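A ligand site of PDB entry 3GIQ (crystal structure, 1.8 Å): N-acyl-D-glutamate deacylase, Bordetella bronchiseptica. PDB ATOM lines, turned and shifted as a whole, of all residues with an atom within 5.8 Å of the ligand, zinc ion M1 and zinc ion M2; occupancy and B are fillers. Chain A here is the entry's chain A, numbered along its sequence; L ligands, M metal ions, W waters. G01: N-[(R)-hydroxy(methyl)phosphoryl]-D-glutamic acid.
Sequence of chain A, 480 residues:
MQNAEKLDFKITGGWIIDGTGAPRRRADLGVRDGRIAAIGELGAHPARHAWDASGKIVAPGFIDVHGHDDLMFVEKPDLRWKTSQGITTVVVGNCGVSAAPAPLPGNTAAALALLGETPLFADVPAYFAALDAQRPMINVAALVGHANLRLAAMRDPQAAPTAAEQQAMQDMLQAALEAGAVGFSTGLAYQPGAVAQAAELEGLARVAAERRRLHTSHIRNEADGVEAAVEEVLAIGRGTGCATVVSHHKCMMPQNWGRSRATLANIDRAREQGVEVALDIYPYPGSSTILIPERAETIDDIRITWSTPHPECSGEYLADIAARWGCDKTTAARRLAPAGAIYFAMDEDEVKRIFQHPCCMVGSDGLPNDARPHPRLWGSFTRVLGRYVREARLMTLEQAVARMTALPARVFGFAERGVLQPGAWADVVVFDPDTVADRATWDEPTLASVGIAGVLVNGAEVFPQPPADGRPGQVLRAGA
Water W1 lies within hydrogen-bond range of an oxygen (OE2) of the ligand, the side-chain carboxylate of Glu 222 and a ring nitrogen (NE2) of His 218.
The side-chain amino group (NZ) of Lys 250 is in salt-bridge range of an oxygen (OXT) of the ligand.
An oxygen (OPA) of the ligand sits close to the side-chain carboxylate (OD2) of Asp 365 (2.6 Å).
O of Ser 288 is in hydrogen-bond range of N of the ligand, at 2.8 Å.
The side-chain hydroxyl (OH) of Tyr 190 sits close to an oxygen (OPB) of the ligand (2.7 Å).
NH1 of Arg 376 lies within salt-bridge range of O of the ligand (2.7 Å).
The side-chain hydroxyl (OG) of Ser 287 lies within hydrogen-bond range of an oxygen (OE1) of the ligand (2.7 Å).
OH of Tyr 282 is in hydrogen-bond range of OXT of the ligand (2.7 Å).
The guanidinium group of Arg 295 lies within salt-bridge range of an oxygen (OE2) of the ligand, 2.7 Å away.
The backbone NH (N) of Ser 288 sits at hydrogen-bond distance from an oxygen (O) of the ligand (2.8 Å).
SD of Met 252 sits close to OE1 of the ligand, at 3.7 Å.
Residues that only touch the ligand: Leu 114, Glu 222, Thr 289 and Tyr 343.
Hydrophobic or aromatic side chains that line the ligand: Leu 114, Tyr 190, His 218, His 248, Met 252, Tyr 282 and Tyr 343.
Of the 26 residues printed, 18 come within 4 Å of the ligand.
The nearest printed residue that does not touch the ligand is Leu 367 (4.3 Å).
Zinc ion M1 is bound by a ring nitrogen (ND1) of His 218 (2.0 Å), an oxygen (OPB) of the ligand (2.0 Å), a ring nitrogen (NE2) of His 248 (2.2 Å) and the side-chain sulfur of Cys 95 (2.3 Å).
Zinc ion M1 has four donor atoms within binding distance.
Zinc ion M2 is bound by a ring nitrogen (NE2) of His 68 (2.0 Å).
Zinc ion M2 is bound by OPA of the ligand (2.0 Å).
Zinc ion M2 is bound by NE2 of His 66 (2.1 Å).
Zinc ion M2 is bound by SG of Cys 95, 2.4 Å away.
The side-chain hydroxyl (OH) of Tyr 343 lies within hydrogen-bond range of the backbone NH (N) of Ile 292.
The backbone NH (N) of Ser 287 is in hydrogen-bond range of the backbone carbonyl oxygen (O) of Tyr 343 (2.8 Å).
A ring nitrogen (ND1) of His 248 is in hydrogen-bond range of the side-chain carboxylate (OE2) of Glu 222 (3.1 Å).
The side-chain amino group (NZ) of Lys 250 lies within hydrogen-bond range of the backbone carbonyl oxygen (O) of His 248 (2.8 Å).
OD1 of Asp 365 sits close to NE2 of His 68 (3.2 Å).
The backbone carbonyl oxygen (O) of His 66 sits at hydrogen-bond distance from the backbone NH (N) of Asp 365.
The side-chain amino group (NZ) of Lys 250 lies within salt-bridge range of the side-chain carboxylate (OE1) of Glu 222 (2.8 Å).
OH of Tyr 282 sits close to NH1 of Arg 376, at 3.4 Å.
Of the 26 residues printed, 3 come within 4 Å of zinc ion M1.
Merely in contact with zinc ion M2: Asp 365 (2.9 Å).
Four residues have an atom within 4 Å of zinc ion M2: His 66, His 68, Cys 95 and Asp 365.
The nearest printed residue that does not touch zinc ion M2 is His 248 (4.03 Å).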
ATOM      1  N   HIS A  66      -5.164  -3.544  -2.359  1.00  0.00           N
ATOM      2  CA  HIS A  66      -4.234  -3.929  -1.311  1.00  0.00           C
ATOM      3  C   HIS A  66      -4.416  -3.104  -0.042  1.00  0.00           C
ATOM      4  O   HIS A  66      -3.625  -2.210   0.256  1.00  0.00           O
ATOM      5  CB  HIS A  66      -2.781  -3.808  -1.779  1.00  0.00           C
ATOM      6  CG  HIS A  66      -1.827  -4.596  -0.934  1.00  0.00           C
ATOM      7  ND1 HIS A  66      -1.419  -5.872  -1.277  1.00  0.00           N
ATOM      8  CD2 HIS A  66      -1.276  -4.336   0.275  1.00  0.00           C
ATOM      9  CE1 HIS A  66      -0.647  -6.356  -0.311  1.00  0.00           C
ATOM     10  NE2 HIS A  66      -0.551  -5.439   0.639  1.00  0.00           N
ATOM     11  N   GLY A  67      -5.474  -3.408   0.689  1.00  0.00           N
ATOM     12  CA  GLY A  67      -5.730  -2.691   1.925  1.00  0.00           C
ATOM     13  C   GLY A  67      -5.407  -3.525   3.158  1.00  0.00           C
ATOM     14  O   GLY A  67      -5.355  -4.760   3.097  1.00  0.00           O
ATOM     15  N   HIS A  68      -5.156  -2.831   4.263  1.00  0.00           N
ATOM     16  CA  HIS A  68      -4.880  -3.471   5.548  1.00  0.00           C
ATOM     17  C   HIS A  68      -5.798  -2.787   6.564  1.00  0.00           C
ATOM     18  O   HIS A  68      -5.462  -2.670   7.747  1.00  0.00           O
ATOM     19  CB  HIS A  68      -3.409  -3.278   5.946  1.00  0.00           C
ATOM     20  CG  HIS A  68      -2.467  -4.213   5.256  1.00  0.00           C
ATOM     21  ND1 HIS A  68      -2.554  -5.581   5.361  1.00  0.00           N
ATOM     22  CD2 HIS A  68      -1.424  -3.968   4.418  1.00  0.00           C
ATOM     23  CE1 HIS A  68      -1.607  -6.139   4.630  1.00  0.00           C
ATOM     24  NE2 HIS A  68      -0.913  -5.188   4.042  1.00  0.00           N
ATOM     25  N   ASN A  94      -4.759  -8.738   3.442  1.00  0.00           N
ATOM     26  CA  ASN A  94      -3.592  -9.006   2.613  1.00  0.00           C
ATOM     27  C   ASN A  94      -2.320  -9.438   3.347  1.00  0.00           C
ATOM     28  O   ASN A  94      -2.224  -9.332   4.567  1.00  0.00           O
ATOM     29  CB  ASN A  94      -3.274  -7.756   1.768  1.00  0.00           C
ATOM     30  CG  ASN A  94      -4.250  -7.577   0.623  1.00  0.00           C
ATOM     31  OD1 ASN A  94      -4.177  -8.291  -0.373  1.00  0.00           O
ATOM     32  ND2 ASN A  94      -5.175  -6.639   0.760  1.00  0.00           N
ATOM     33  N   CYS A  95      -1.355  -9.926   2.580  1.00  0.00           N
ATOM     34  CA  CYS A  95      -0.057 -10.352   3.097  1.00  0.00           C
ATOM     35  C   CYS A  95      -0.078 -11.379   4.230  1.00  0.00           C
ATOM     36  O   CYS A  95       0.796 -11.371   5.101  1.00  0.00           O
ATOM     37  CB  CYS A  95       0.730  -9.117   3.530  1.00  0.00           C
ATOM     38  SG  CYS A  95       0.896  -7.927   2.178  1.00  0.00           S
ATOM     39  N   LEU A 114      -0.009  -4.735  12.762  1.00  0.00           N
ATOM     40  CA  LEU A 114      -0.256  -3.668  11.797  1.00  0.00           C
ATOM     41  C   LEU A 114      -1.738  -3.425  11.521  1.00  0.00           C
ATOM     42  O   LEU A 114      -2.114  -2.347  11.058  1.00  0.00           O
ATOM     43  CB  LEU A 114       0.455  -3.973  10.477  1.00  0.00           C
ATOM     44  CG  LEU A 114       1.985  -3.992  10.508  1.00  0.00           C
ATOM     45  CD1 LEU A 114       2.507  -4.281   9.093  1.00  0.00           C
ATOM     46  CD2 LEU A 114       2.501  -2.654  11.005  1.00  0.00           C
ATOM     47  N   ALA A 189       7.289 -13.843   3.377  1.00  0.00           N
ATOM     48  CA  ALA A 189       8.510 -13.198   3.846  1.00  0.00           C
ATOM     49  C   ALA A 189       8.439 -12.992   5.356  1.00  0.00           C
ATOM     50  O   ALA A 189       9.382 -12.500   5.973  1.00  0.00           O
ATOM     51  CB  ALA A 189       8.704 -11.858   3.137  1.00  0.00           C
ATOM     52  N   TYR A 190       7.301 -13.366   5.946  1.00  0.00           N
ATOM     53  CA  TYR A 190       7.058 -13.203   7.382  1.00  0.00           C
ATOM     54  C   TYR A 190       6.768 -14.521   8.097  1.00  0.00           C
ATOM     55  O   TYR A 190       6.389 -15.511   7.476  1.00  0.00           O
ATOM     56  CB  TYR A 190       5.829 -12.318   7.625  1.00  0.00           C
ATOM     57  CG  TYR A 190       5.847 -10.949   6.991  1.00  0.00           C
ATOM     58  CD1 TYR A 190       6.804 -10.001   7.343  1.00  0.00           C
ATOM     59  CD2 TYR A 190       4.850 -10.570   6.086  1.00  0.00           C
ATOM     60  CE1 TYR A 190       6.765  -8.705   6.829  1.00  0.00           C
ATOM     61  CE2 TYR A 190       4.796  -9.279   5.565  1.00  0.00           C
ATOM     62  CZ  TYR A 190       5.756  -8.352   5.947  1.00  0.00           C
ATOM     63  OH  TYR A 190       5.701  -7.063   5.467  1.00  0.00           O
ATOM     64  N   HIS A 218       2.335 -12.063  -0.858  1.00  0.00           N
ATOM     65  CA  HIS A 218       3.463 -11.210  -0.538  1.00  0.00           C
ATOM     66  C   HIS A 218       4.477 -12.347  -0.637  1.00  0.00           C
ATOM     67  O   HIS A 218       4.544 -13.210   0.244  1.00  0.00           O
ATOM     68  CB  HIS A 218       3.386 -10.693   0.896  1.00  0.00           C
ATOM     69  CG  HIS A 218       4.627  -9.978   1.330  1.00  0.00           C
ATOM     70  ND1 HIS A 218       4.595  -8.849   2.118  1.00  0.00           N
ATOM     71  CD2 HIS A 218       5.929 -10.235   1.091  1.00  0.00           C
ATOM     72  CE1 HIS A 218       5.833  -8.438   2.349  1.00  0.00           C
ATOM     73  NE2 HIS A 218       6.662  -9.266   1.739  1.00  0.00           N
ATOM     74  N   GLU A 222      11.715 -10.241  -1.705  1.00  0.00           N
ATOM     75  CA  GLU A 222      11.597  -9.224  -2.736  1.00  0.00           C
ATOM     76  C   GLU A 222      12.914  -8.506  -3.018  1.00  0.00           C
ATOM     77  O   GLU A 222      12.936  -7.412  -3.568  1.00  0.00           O
ATOM     78  CB  GLU A 222      10.507  -8.214  -2.351  1.00  0.00           C
ATOM     79  CG  GLU A 222       9.149  -8.880  -2.159  1.00  0.00           C
ATOM     80  CD  GLU A 222       8.022  -7.897  -1.956  1.00  0.00           C
ATOM     81  OE1 GLU A 222       8.027  -7.182  -0.932  1.00  0.00           O
ATOM     82  OE2 GLU A 222       7.132  -7.826  -2.826  1.00  0.00           O
ATOM     83  N   SER A 247       1.292  -9.418  -4.863  1.00  0.00           N
ATOM     84  CA  SER A 247       1.107  -8.184  -4.118  1.00  0.00           C
ATOM     85  C   SER A 247       2.310  -7.262  -4.140  1.00  0.00           C
ATOM     86  O   SER A 247       3.455  -7.716  -4.171  1.00  0.00           O
ATOM     87  CB  SER A 247       0.772  -8.503  -2.649  1.00  0.00           C
ATOM     88  OG  SER A 247      -0.397  -9.296  -2.556  1.00  0.00           O
ATOM     89  N   HIS A 248       2.034  -5.959  -4.122  1.00  0.00           N
ATOM     90  CA  HIS A 248       3.063  -4.913  -4.136  1.00  0.00           C
ATOM     91  C   HIS A 248       4.368  -5.374  -4.768  1.00  0.00           C
ATOM     92  O   HIS A 248       5.423  -5.380  -4.128  1.00  0.00           O
ATOM     93  CB  HIS A 248       3.314  -4.403  -2.708  1.00  0.00           C
ATOM     94  CG  HIS A 248       3.545  -5.481  -1.692  1.00  0.00           C
ATOM     95  ND1 HIS A 248       4.513  -6.462  -1.838  1.00  0.00           N
ATOM     96  CD2 HIS A 248       2.964  -5.711  -0.490  1.00  0.00           C
ATOM     97  CE1 HIS A 248       4.512  -7.239  -0.771  1.00  0.00           C
ATOM     98  NE2 HIS A 248       3.586  -6.805   0.062  1.00  0.00           N
ATOM     99  N   LYS A 250       7.776  -5.568  -6.485  1.00  0.00           N
ATOM    100  CA  LYS A 250       8.900  -4.638  -6.439  1.00  0.00           C
ATOM    101  C   LYS A 250      10.218  -5.394  -6.447  1.00  0.00           C
ATOM    102  O   LYS A 250      10.246  -6.625  -6.365  1.00  0.00           O
ATOM    103  CB  LYS A 250       8.832  -3.856  -5.121  1.00  0.00           C
ATOM    104  CG  LYS A 250       9.071  -4.773  -3.915  1.00  0.00           C
ATOM    105  CD  LYS A 250       9.155  -4.026  -2.586  1.00  0.00           C
ATOM    106  CE  LYS A 250       7.793  -3.579  -2.092  1.00  0.00           C
ATOM    107  NZ  LYS A 250       6.877  -4.742  -1.851  1.00  0.00           N
ATOM    108  N   MET A 252      13.759  -4.847  -4.339  1.00  0.00           N
ATOM    109  CA  MET A 252      14.463  -4.105  -3.303  1.00  0.00           C
ATOM    110  C   MET A 252      15.984  -4.274  -3.341  1.00  0.00           C
ATOM    111  O   MET A 252      16.486  -5.362  -3.630  1.00  0.00           O
ATOM    112  CB  MET A 252      13.951  -4.513  -1.921  1.00  0.00           C
ATOM    113  CG  MET A 252      12.487  -4.191  -1.704  1.00  0.00           C
ATOM    114  SD  MET A 252      11.918  -4.703  -0.072  1.00  0.00           S
ATOM    115  CE  MET A 252      12.615  -3.387   0.932  1.00  0.00           C
ATOM    116  N   TYR A 282       2.104   0.313  -5.348  1.00  0.00           N
ATOM    117  CA  TYR A 282       1.745   1.605  -4.788  1.00  0.00           C
ATOM    118  C   TYR A 282       2.838   2.442  -5.472  1.00  0.00           C
ATOM    119  O   TYR A 282       3.961   1.965  -5.677  1.00  0.00           O
ATOM    120  CB  TYR A 282       1.843   1.626  -3.261  1.00  0.00           C
ATOM    121  CG  TYR A 282       3.054   0.938  -2.673  1.00  0.00           C
ATOM    122  CD1 TYR A 282       4.283   1.590  -2.590  1.00  0.00           C
ATOM    123  CD2 TYR A 282       2.949  -0.364  -2.176  1.00  0.00           C
ATOM    124  CE1 TYR A 282       5.389   0.959  -2.024  1.00  0.00           C
ATOM    125  CE2 TYR A 282       4.047  -1.000  -1.606  1.00  0.00           C
ATOM    126  CZ  TYR A 282       5.259  -0.322  -1.529  1.00  0.00           C
ATOM    127  OH  TYR A 282       6.338  -0.943  -0.955  1.00  0.00           O
ATOM    128  N   GLY A 286       9.619   3.533  -1.663  1.00  0.00           N
ATOM    129  CA  GLY A 286       9.914   3.156  -0.297  1.00  0.00           C
ATOM    130  C   GLY A 286       8.817   2.231   0.184  1.00  0.00           C
ATOM    131  O   GLY A 286       7.648   2.456  -0.113  1.00  0.00           O
ATOM    132  N   SER A 287       9.177   1.172   0.908  1.00  0.00           N
ATOM    133  CA  SER A 287       8.165   0.242   1.423  1.00  0.00           C
ATOM    134  C   SER A 287       7.894   0.582   2.885  1.00  0.00           C
ATOM    135  O   SER A 287       8.459   1.517   3.425  1.00  0.00           O
ATOM    136  CB  SER A 287       8.657  -1.199   1.299  1.00  0.00           C
ATOM    137  OG  SER A 287       9.781  -1.428   2.142  1.00  0.00           O
ATOM    138  N   SER A 288       7.007  -0.182   3.509  1.00  0.00           N
ATOM    139  CA  SER A 288       6.691   0.050   4.922  1.00  0.00           C
ATOM    140  C   SER A 288       6.044  -1.177   5.538  1.00  0.00           C
ATOM    141  O   SER A 288       5.070  -1.720   5.020  1.00  0.00           O
ATOM    142  CB  SER A 288       5.773   1.258   5.081  1.00  0.00           C
ATOM    143  OG  SER A 288       5.551   1.536   6.458  1.00  0.00           O
ATOM    144  N   THR A 289       6.605  -1.619   6.664  1.00  0.00           N
ATOM    145  CA  THR A 289       6.090  -2.777   7.377  1.00  0.00           C
ATOM    146  C   THR A 289       6.708  -2.752   8.774  1.00  0.00           C
ATOM    147  O   THR A 289       7.088  -1.682   9.248  1.00  0.00           O
ATOM    148  CB  THR A 289       6.455  -4.097   6.644  1.00  0.00           C
ATOM    149  OG1 THR A 289       5.834  -5.207   7.303  1.00  0.00           O
ATOM    150  CG2 THR A 289       7.962  -4.305   6.613  1.00  0.00           C
ATOM    151  N   ILE A 292      12.574  -4.338  10.987  1.00  0.00           N
ATOM    152  CA  ILE A 292      13.374  -5.554  10.927  1.00  0.00           C
ATOM    153  C   ILE A 292      14.823  -5.203  11.209  1.00  0.00           C
ATOM    154  O   ILE A 292      15.521  -4.656  10.357  1.00  0.00           O
ATOM    155  CB  ILE A 292      13.258  -6.195   9.527  1.00  0.00           C
ATOM    156  CG1 ILE A 292      11.795  -6.544   9.245  1.00  0.00           C
ATOM    157  CG2 ILE A 292      14.141  -7.434   9.436  1.00  0.00           C
ATOM    158  CD1 ILE A 292      11.513  -6.894   7.779  1.00  0.00           C
ATOM    159  N   ARG A 295      17.911  -5.440   8.924  1.00  0.00           N
ATOM    160  CA  ARG A 295      18.064  -4.485   7.822  1.00  0.00           C
ATOM    161  C   ARG A 295      18.788  -3.200   8.234  1.00  0.00           C
ATOM    162  O   ARG A 295      19.115  -2.375   7.389  1.00  0.00           O
ATOM    163  CB  ARG A 295      16.688  -4.103   7.260  1.00  0.00           C
ATOM    164  CG  ARG A 295      15.949  -5.243   6.598  1.00  0.00           C
ATOM    165  CD  ARG A 295      14.612  -4.754   6.047  1.00  0.00           C
ATOM    166  NE  ARG A 295      13.921  -5.787   5.278  1.00  0.00           N
ATOM    167  CZ  ARG A 295      12.780  -5.597   4.639  1.00  0.00           C
ATOM    168  NH1 ARG A 295      12.184  -4.410   4.674  1.00  0.00           N
ATOM    169  NH2 ARG A 295      12.231  -6.582   3.943  1.00  0.00           N
ATOM    170  N   TYR A 343      11.208   1.784   4.394  1.00  0.00           N
ATOM    171  CA  TYR A 343      12.481   1.396   3.797  1.00  0.00           C
ATOM    172  C   TYR A 343      12.600   1.936   2.378  1.00  0.00           C
ATOM    173  O   TYR A 343      11.865   1.504   1.491  1.00  0.00           O
ATOM    174  CB  TYR A 343      12.570  -0.136   3.769  1.00  0.00           C
ATOM    175  CG  TYR A 343      12.367  -0.803   5.121  1.00  0.00           C
ATOM    176  CD1 TYR A 343      13.421  -0.969   6.012  1.00  0.00           C
ATOM    177  CD2 TYR A 343      11.105  -1.299   5.487  1.00  0.00           C
ATOM    178  CE1 TYR A 343      13.246  -1.604   7.242  1.00  0.00           C
ATOM    179  CE2 TYR A 343      10.915  -1.942   6.727  1.00  0.00           C
ATOM    180  CZ  TYR A 343      11.994  -2.086   7.595  1.00  0.00           C
ATOM    181  OH  TYR A 343      11.838  -2.744   8.790  1.00  0.00           O
ATOM    182  N   MET A 346      13.801   0.957  -3.328  1.00  0.00           N
ATOM    183  CA  MET A 346      13.418   0.661  -4.697  1.00  0.00           C
ATOM    184  C   MET A 346      13.801   1.772  -5.668  1.00  0.00           C
ATOM    185  O   MET A 346      14.105   2.890  -5.264  1.00  0.00           O
ATOM    186  CB  MET A 346      11.915   0.394  -4.794  1.00  0.00           C
ATOM    187  CG  MET A 346      11.443  -0.850  -4.040  1.00  0.00           C
ATOM    188  SD  MET A 346      10.866  -0.518  -2.366  1.00  0.00           S
ATOM    189  CE  MET A 346       9.194   0.003  -2.695  1.00  0.00           C
ATOM    190  N   ASP A 365      -1.750  -0.044  -0.007  1.00  0.00           N
ATOM    191  CA  ASP A 365      -0.994  -0.704   1.057  1.00  0.00           C
ATOM    192  C   ASP A 365      -0.848   0.238   2.254  1.00  0.00           C
ATOM    193  O   ASP A 365       0.164   0.238   2.958  1.00  0.00           O
ATOM    194  CB  ASP A 365       0.375  -1.147   0.559  1.00  0.00           C
ATOM    195  CG  ASP A 365       0.976  -2.258   1.414  1.00  0.00           C
ATOM    196  OD1 ASP A 365       0.286  -2.747   2.335  1.00  0.00           O
ATOM    197  OD2 ASP A 365       2.142  -2.646   1.169  1.00  0.00           O
ATOM    198  N   LEU A 367      -1.129   1.724   5.911  1.00  0.00           N
ATOM    199  CA  LEU A 367      -1.086   1.115   7.239  1.00  0.00           C
ATOM    200  C   LEU A 367      -1.719   2.171   8.145  1.00  0.00           C
ATOM    201  O   LEU A 367      -1.027   2.970   8.783  1.00  0.00           O
ATOM    202  CB  LEU A 367       0.358   0.830   7.633  1.00  0.00           C
ATOM    203  CG  LEU A 367       1.072  -0.133   6.665  1.00  0.00           C
ATOM    204  CD1 LEU A 367       2.491  -0.389   7.130  1.00  0.00           C
ATOM    205  CD2 LEU A 367       0.296  -1.434   6.574  1.00  0.00           C
ATOM    206  N   ARG A 376       1.551   6.760   1.278  1.00  0.00           N
ATOM    207  CA  ARG A 376       0.711   5.991   0.358  1.00  0.00           C
ATOM    208  C   ARG A 376      -0.674   5.775   0.950  1.00  0.00           C
ATOM    209  O   ARG A 376      -1.640   5.524   0.226  1.00  0.00           O
ATOM    210  CB  ARG A 376       1.364   4.637   0.063  1.00  0.00           C
ATOM    211  CG  ARG A 376       1.428   3.702   1.254  1.00  0.00           C
ATOM    212  CD  ARG A 376       2.379   2.554   0.988  1.00  0.00           C
ATOM    213  NE  ARG A 376       2.371   1.562   2.065  1.00  0.00           N
ATOM    214  CZ  ARG A 376       3.283   0.615   2.211  1.00  0.00           C
ATOM    215  NH1 ARG A 376       4.302   0.534   1.361  1.00  0.00           N
ATOM    216  NH2 ARG A 376       3.189  -0.259   3.200  1.00  0.00           N
HETATM  217  CD  G01 L   1       9.382  -5.030   2.644  1.00  0.00           C
HETATM  218  CG  G01 L   1       8.052  -4.870   1.909  1.00  0.00           C
HETATM  219  CB  G01 L   1       6.951  -4.488   2.897  1.00  0.00           C
HETATM  220  CA  G01 L   1       5.506  -4.220   2.373  1.00  0.00           C
HETATM  221  C   G01 L   1       5.539  -3.010   1.412  1.00  0.00           C
HETATM  222  C6  G01 L   1       2.692  -4.730   5.366  1.00  0.00           C
HETATM  223  P   G01 L   1       3.318  -5.067   3.730  1.00  0.00           P
HETATM  224  OPA G01 L   1       2.136  -4.773   2.709  1.00  0.00           O
HETATM  225  OPB G01 L   1       3.740  -6.493   3.653  1.00  0.00           O
HETATM  226  N   G01 L   1       4.487  -3.979   3.443  1.00  0.00           N
HETATM  227  O   G01 L   1       5.423  -1.865   1.883  1.00  0.00           O
HETATM  228  OXT G01 L   1       5.675  -3.277   0.207  1.00  0.00           O
HETATM  229  OE1 G01 L   1       9.969  -3.981   2.994  1.00  0.00           O
HETATM  230  OE2 G01 L   1       9.762  -6.196   2.853  1.00  0.00           O
HETATM  231 ZN    ZN M   1       3.149  -7.524   2.073  1.00  0.00          ZN
HETATM  232 ZN    ZN M   2       0.322  -5.594   2.548  1.00  0.00          ZN
HETATM  233  O   HOH W   1       9.192  -8.206   1.262  1.00  0.00           O
